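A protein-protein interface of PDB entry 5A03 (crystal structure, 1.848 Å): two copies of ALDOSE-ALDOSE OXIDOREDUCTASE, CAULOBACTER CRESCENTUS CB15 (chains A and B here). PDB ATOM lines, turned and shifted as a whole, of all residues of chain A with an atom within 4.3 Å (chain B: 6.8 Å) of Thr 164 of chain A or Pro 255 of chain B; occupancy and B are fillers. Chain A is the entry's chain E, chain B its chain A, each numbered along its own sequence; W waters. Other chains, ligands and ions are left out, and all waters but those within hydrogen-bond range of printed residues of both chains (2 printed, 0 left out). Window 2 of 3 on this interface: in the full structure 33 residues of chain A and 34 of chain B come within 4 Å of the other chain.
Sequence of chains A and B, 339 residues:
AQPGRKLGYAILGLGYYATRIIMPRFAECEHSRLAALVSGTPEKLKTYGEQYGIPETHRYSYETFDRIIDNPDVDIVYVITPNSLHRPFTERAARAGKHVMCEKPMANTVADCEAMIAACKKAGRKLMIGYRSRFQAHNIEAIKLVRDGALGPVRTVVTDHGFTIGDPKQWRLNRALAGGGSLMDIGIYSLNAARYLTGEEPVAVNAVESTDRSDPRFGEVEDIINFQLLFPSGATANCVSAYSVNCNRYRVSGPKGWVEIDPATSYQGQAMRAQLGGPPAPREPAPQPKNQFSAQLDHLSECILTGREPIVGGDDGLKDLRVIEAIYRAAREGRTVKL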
ATOM      1  N   PHE A 163     -25.210 -15.058  -1.732  1.00  0.00           N
ATOM      2  CA  PHE A 163     -24.218 -16.079  -2.008  1.00  0.00           C
ATOM      3  C   PHE A 163     -24.912 -17.234  -2.683  1.00  0.00           C
ATOM      4  O   PHE A 163     -26.129 -17.388  -2.569  1.00  0.00           O
ATOM      5  CB  PHE A 163     -23.471 -16.527  -0.738  1.00  0.00           C
ATOM      6  CG  PHE A 163     -24.314 -17.318   0.248  1.00  0.00           C
ATOM      7  CD1 PHE A 163     -25.052 -16.672   1.222  1.00  0.00           C
ATOM      8  CD2 PHE A 163     -24.311 -18.712   0.230  1.00  0.00           C
ATOM      9  CE1 PHE A 163     -25.813 -17.394   2.141  1.00  0.00           C
ATOM     10  CE2 PHE A 163     -25.069 -19.440   1.155  1.00  0.00           C
ATOM     11  CZ  PHE A 163     -25.817 -18.775   2.104  1.00  0.00           C
ATOM     12  N   THR A 164     -24.134 -18.025  -3.418  1.00  0.00           N
ATOM     13  CA  THR A 164     -24.653 -19.191  -4.121  1.00  0.00           C
ATOM     14  C   THR A 164     -24.816 -20.325  -3.126  1.00  0.00           C
ATOM     15  O   THR A 164     -23.855 -21.026  -2.822  1.00  0.00           O
ATOM     16  CB  THR A 164     -23.709 -19.630  -5.259  1.00  0.00           C
ATOM     17  OG1 THR A 164     -22.365 -19.654  -4.767  1.00  0.00           O
ATOM     18  CG2 THR A 164     -23.784 -18.661  -6.432  1.00  0.00           C
ATOM     19  N   ILE A 165     -26.025 -20.493  -2.603  1.00  0.00           N
ATOM     20  CA  ILE A 165     -26.252 -21.473  -1.547  1.00  0.00           C
ATOM     21  C   ILE A 165     -26.186 -22.880  -2.150  1.00  0.00           C
ATOM     22  O   ILE A 165     -26.439 -23.060  -3.338  1.00  0.00           O
ATOM     23  CB  ILE A 165     -27.606 -21.216  -0.827  1.00  0.00           C
ATOM     24  CG1 ILE A 165     -27.672 -21.933   0.528  1.00  0.00           C
ATOM     25  CG2 ILE A 165     -28.787 -21.560  -1.724  1.00  0.00           C
ATOM     26  CD1 ILE A 165     -28.808 -21.426   1.425  1.00  0.00           C
ATOM     27  N   GLY A 166     -25.810 -23.865  -1.342  1.00  0.00           N
ATOM     28  CA  GLY A 166     -25.544 -25.197  -1.861  1.00  0.00           C
ATOM     29  C   GLY A 166     -26.587 -26.260  -1.553  1.00  0.00           C
ATOM     30  O   GLY A 166     -27.590 -26.386  -2.257  1.00  0.00           O
ATOM     31  N   TYR A 243     -29.816 -15.856  -3.354  1.00  0.00           N
ATOM     32  CA  TYR A 243     -29.242 -17.157  -3.033  1.00  0.00           C
ATOM     33  C   TYR A 243     -28.600 -17.799  -4.269  1.00  0.00           C
ATOM     34  O   TYR A 243     -28.188 -18.959  -4.235  1.00  0.00           O
ATOM     35  CB  TYR A 243     -30.323 -18.085  -2.468  1.00  0.00           C
ATOM     36  CG  TYR A 243     -30.431 -18.151  -0.952  1.00  0.00           C
ATOM     37  CD1 TYR A 243     -29.404 -17.715  -0.125  1.00  0.00           C
ATOM     38  CD2 TYR A 243     -31.562 -18.696  -0.354  1.00  0.00           C
ATOM     39  CE1 TYR A 243     -29.506 -17.816   1.270  1.00  0.00           C
ATOM     40  CE2 TYR A 243     -31.673 -18.792   1.029  1.00  0.00           C
ATOM     41  CZ  TYR A 243     -30.649 -18.365   1.829  1.00  0.00           C
ATOM     42  OH  TYR A 243     -30.775 -18.482   3.194  1.00  0.00           O
ATOM     43  N   SER A 244     -28.520 -17.059  -5.373  1.00  0.00           N
ATOM     44  CA  SER A 244     -27.989 -17.643  -6.595  1.00  0.00           C
ATOM     45  C   SER A 244     -26.870 -16.813  -7.222  1.00  0.00           C
ATOM     46  O   SER A 244     -26.384 -17.146  -8.302  1.00  0.00           O
ATOM     47  CB  SER A 244     -29.109 -17.854  -7.618  1.00  0.00           C
ATOM     48  OG  SER A 244     -29.779 -16.643  -7.904  1.00  0.00           O
ATOM     49  N   VAL A 245     -26.477 -15.730  -6.560  1.00  0.00           N
ATOM     50  CA  VAL A 245     -25.289 -14.991  -6.968  1.00  0.00           C
ATOM     51  C   VAL A 245     -24.489 -14.594  -5.750  1.00  0.00           C
ATOM     52  O   VAL A 245     -25.001 -14.575  -4.627  1.00  0.00           O
ATOM     53  CB  VAL A 245     -25.614 -13.719  -7.784  1.00  0.00           C
ATOM     54  CG1 VAL A 245     -26.406 -14.053  -9.032  1.00  0.00           C
ATOM     55  CG2 VAL A 245     -26.342 -12.705  -6.925  1.00  0.00           C
ATOM     56  N   ASN A 246     -23.218 -14.291  -5.983  1.00  0.00           N
ATOM     57  CA  ASN A 246     -22.327 -13.844  -4.935  1.00  0.00           C
ATOM     58  C   ASN A 246     -22.141 -12.340  -4.983  1.00  0.00           C
ATOM     59  O   ASN A 246     -21.677 -11.781  -5.994  1.00  0.00           O
ATOM     60  CB  ASN A 246     -20.973 -14.549  -5.061  1.00  0.00           C
ATOM     61  CG  ASN A 246     -21.052 -16.026  -4.714  1.00  0.00           C
ATOM     62  OD1 ASN A 246     -21.469 -16.394  -3.612  1.00  0.00           O
ATOM     63  ND2 ASN A 246     -20.653 -16.882  -5.654  1.00  0.00           N
ATOM     64  N   ALA B 150     -20.466 -17.160 -19.732  1.00  0.00           N
ATOM     65  CA  ALA B 150     -19.419 -17.108 -18.711  1.00  0.00           C
ATOM     66  C   ALA B 150     -19.974 -16.905 -17.303  1.00  0.00           C
ATOM     67  O   ALA B 150     -19.333 -17.279 -16.322  1.00  0.00           O
ATOM     68  CB  ALA B 150     -18.419 -16.002 -19.032  1.00  0.00           C
ATOM     69  N   LEU B 151     -21.159 -16.304 -17.207  1.00  0.00           N
ATOM     70  CA  LEU B 151     -21.784 -16.025 -15.910  1.00  0.00           C
ATOM     71  C   LEU B 151     -22.838 -17.059 -15.536  1.00  0.00           C
ATOM     72  O   LEU B 151     -23.319 -17.085 -14.394  1.00  0.00           O
ATOM     73  CB  LEU B 151     -22.448 -14.635 -15.917  1.00  0.00           C
ATOM     74  CG  LEU B 151     -21.667 -13.399 -16.365  1.00  0.00           C
ATOM     75  CD1 LEU B 151     -22.482 -12.122 -16.120  1.00  0.00           C
ATOM     76  CD2 LEU B 151     -20.327 -13.312 -15.654  1.00  0.00           C
ATOM     77  N   GLY B 152     -23.197 -17.901 -16.497  1.00  0.00           N
ATOM     78  CA  GLY B 152     -24.430 -18.665 -16.423  1.00  0.00           C
ATOM     79  C   GLY B 152     -25.582 -17.716 -16.726  1.00  0.00           C
ATOM     80  O   GLY B 152     -25.363 -16.615 -17.226  1.00  0.00           O
ATOM     81  N   PRO B 153     -26.822 -18.128 -16.430  1.00  0.00           N
ATOM     82  CA  PRO B 153     -27.940 -17.216 -16.704  1.00  0.00           C
ATOM     83  C   PRO B 153     -27.828 -15.913 -15.915  1.00  0.00           C
ATOM     84  O   PRO B 153     -27.466 -15.934 -14.739  1.00  0.00           O
ATOM     85  CB  PRO B 153     -29.174 -18.018 -16.254  1.00  0.00           C
ATOM     86  CG  PRO B 153     -28.713 -19.437 -16.185  1.00  0.00           C
ATOM     87  CD  PRO B 153     -27.271 -19.373 -15.790  1.00  0.00           C
ATOM     88  N   VAL B 154     -28.127 -14.785 -16.552  1.00  0.00           N
ATOM     89  CA  VAL B 154     -28.123 -13.522 -15.828  1.00  0.00           C
ATOM     90  C   VAL B 154     -29.186 -13.539 -14.743  1.00  0.00           C
ATOM     91  O   VAL B 154     -30.374 -13.783 -15.018  1.00  0.00           O
ATOM     92  CB  VAL B 154     -28.361 -12.321 -16.752  1.00  0.00           C
ATOM     93  CG1 VAL B 154     -28.428 -11.013 -15.935  1.00  0.00           C
ATOM     94  CG2 VAL B 154     -27.246 -12.237 -17.774  1.00  0.00           C
ATOM     95  N   ARG B 155     -28.755 -13.293 -13.512  1.00  0.00           N
ATOM     96  CA  ARG B 155     -29.682 -13.210 -12.394  1.00  0.00           C
ATOM     97  C   ARG B 155     -29.911 -11.753 -11.974  1.00  0.00           C
ATOM     98  O   ARG B 155     -31.047 -11.342 -11.758  1.00  0.00           O
ATOM     99  CB  ARG B 155     -29.171 -14.033 -11.216  1.00  0.00           C
ATOM    100  CG  ARG B 155     -28.934 -15.511 -11.547  1.00  0.00           C
ATOM    101  CD  ARG B 155     -30.253 -16.215 -11.873  1.00  0.00           C
ATOM    102  NE  ARG B 155     -31.119 -16.327 -10.701  1.00  0.00           N
ATOM    103  CZ  ARG B 155     -32.412 -16.007 -10.687  1.00  0.00           C
ATOM    104  NH1 ARG B 155     -32.984 -15.548 -11.794  1.00  0.00           N
ATOM    105  NH2 ARG B 155     -33.140 -16.151  -9.575  1.00  0.00           N
ATOM    106  N   SER B 253     -24.480 -10.160 -12.896  1.00  0.00           N
ATOM    107  CA  SER B 253     -24.113 -11.343 -12.108  1.00  0.00           C
ATOM    108  C   SER B 253     -24.962 -12.563 -12.459  1.00  0.00           C
ATOM    109  O   SER B 253     -26.168 -12.458 -12.681  1.00  0.00           O
ATOM    110  CB  SER B 253     -24.267 -11.062 -10.606  1.00  0.00           C
ATOM    111  OG  SER B 253     -23.614  -9.866 -10.201  1.00  0.00           O
ATOM    112  N   GLY B 254     -24.319 -13.723 -12.480  1.00  0.00           N
ATOM    113  CA  GLY B 254     -25.001 -14.984 -12.645  1.00  0.00           C
ATOM    114  C   GLY B 254     -24.406 -15.955 -11.638  1.00  0.00           C
ATOM    115  O   GLY B 254     -23.490 -15.593 -10.901  1.00  0.00           O
ATOM    116  N   PRO B 255     -24.895 -17.207 -11.629  1.00  0.00           N
ATOM    117  CA  PRO B 255     -24.431 -18.197 -10.647  1.00  0.00           C
ATOM    118  C   PRO B 255     -22.955 -18.540 -10.803  1.00  0.00           C
ATOM    119  O   PRO B 255     -22.344 -18.992  -9.844  1.00  0.00           O
ATOM    120  CB  PRO B 255     -25.312 -19.425 -10.925  1.00  0.00           C
ATOM    121  CG  PRO B 255     -25.843 -19.223 -12.308  1.00  0.00           C
ATOM    122  CD  PRO B 255     -25.915 -17.745 -12.543  1.00  0.00           C
ATOM    123  N   LYS B 256     -22.377 -18.314 -11.978  1.00  0.00           N
ATOM    124  CA  LYS B 256     -20.970 -18.675 -12.168  1.00  0.00           C
ATOM    125  C   LYS B 256     -20.019 -17.497 -11.950  1.00  0.00           C
ATOM    126  O   LYS B 256     -18.800 -17.664 -11.901  1.00  0.00           O
ATOM    127  CB  LYS B 256     -20.771 -19.273 -13.561  1.00  0.00           C
ATOM    128  CG  LYS B 256     -21.654 -20.493 -13.802  1.00  0.00           C
ATOM    129  CD  LYS B 256     -21.151 -21.347 -14.952  1.00  0.00           C
ATOM    130  CE  LYS B 256     -21.267 -20.622 -16.261  1.00  0.00           C
ATOM    131  NZ  LYS B 256     -20.405 -21.218 -17.330  1.00  0.00           N
ATOM    132  N   GLY B 257     -20.568 -16.299 -11.796  1.00  0.00           N
ATOM    133  CA  GLY B 257     -19.710 -15.148 -11.601  1.00  0.00           C
ATOM    134  C   GLY B 257     -20.319 -13.835 -12.043  1.00  0.00           C
ATOM    135  O   GLY B 257     -21.512 -13.759 -12.347  1.00  0.00           O
HETATM  136  O   HOH W   1     -22.114 -14.493  -8.680  1.00  0.00           O
HETATM  137  O   HOH W   2     -22.499  -9.708  -7.616  1.00  0.00           O
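The guanidinium group (NE) of Arg 155 of chain B sits at hydrogen-bond distance from the side-chain hydroxyl (OG) of Ser 244 of chain A (3.1 Å).
Of the 8 printed residues of chain A, 3 touch a printed residue of chain B. Of the 11 printed residues of chain B, 4 touch a printed residue of chain A. Printed residues of chain B that touch a printed residue of chain A: Arg 155, Ser 253, Gly 254 and Pro 255. Along chain B the printed residues that touch a printed residue of chain A span positions 155 to 255.
Among the printed residues, pairs that only touch across the chains: Ser 244 of chain A with Pro 255 of chain B, Val 245 of chain A with Arg 155 of chain B, Thr 164 of chain A with Pro 255 of chain B, Val 245 of chain A with Gly 254 of chain B and Val 245 of chain A with Ser 253 of chain B.
O of Ser 253 of chain B sits at hydrogen-bond distance from N of Arg 155 of chain B. The backbone NH of Phe 163 of chain A is in hydrogen-bond range of the backbone carbonyl oxygen of Val 245 of chain A (2.9 Å). The backbone NH of Thr 164 of chain A is in hydrogen-bond range of the side-chain amide oxygen of Asn 246 of chain A (3.1 Å).
Water W2 bridges O of Asn 246 of chain A (2.8 Å) and OG of Ser 253 of chain B (2.8 Å). Water W1 bridges the backbone carbonyl oxygen (O) of Gly 254 of chain B (2.8 Å) and the backbone NH (N) of Asn 246 of chain A (2.9 Å).
No position is printed for both chains. Of the 6 pairs that touch across the chains among the printed residues, none has its exchanged pair printed and touching as well.
Thr 164 of chain A touches one residue of chain B. Of the printed residues of chain B, Ser 244 of chain A touches Arg 155 and Pro 255. Printed residues of chain B within 4 Å of Val 245 of chain A: Arg 155, Ser 253 and Gly 254. Pro 153 of chain B touches none of the printed residues of chain A. Of the printed residues of chain A, Arg 155 of chain B touches Ser 244 and Val 245. Of the printed residues of chain A, Ser 253 of chain B touches Val 245. Of chain A, only Thr 164 (3.7 Å) and Ser 244 (3.2 Å) come within 4 Å of Pro 255 of chain B. Gly 257 of chain B touches none of the printed residues of chain A. The nearest residue of chain B that does not touch Thr 164 of chain A is Gly 254 of chain B (5.4 Å). The nearest printed residue of chain A that does not touch Pro 255 of chain B is Val 245 of chain A (4.4 Å).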
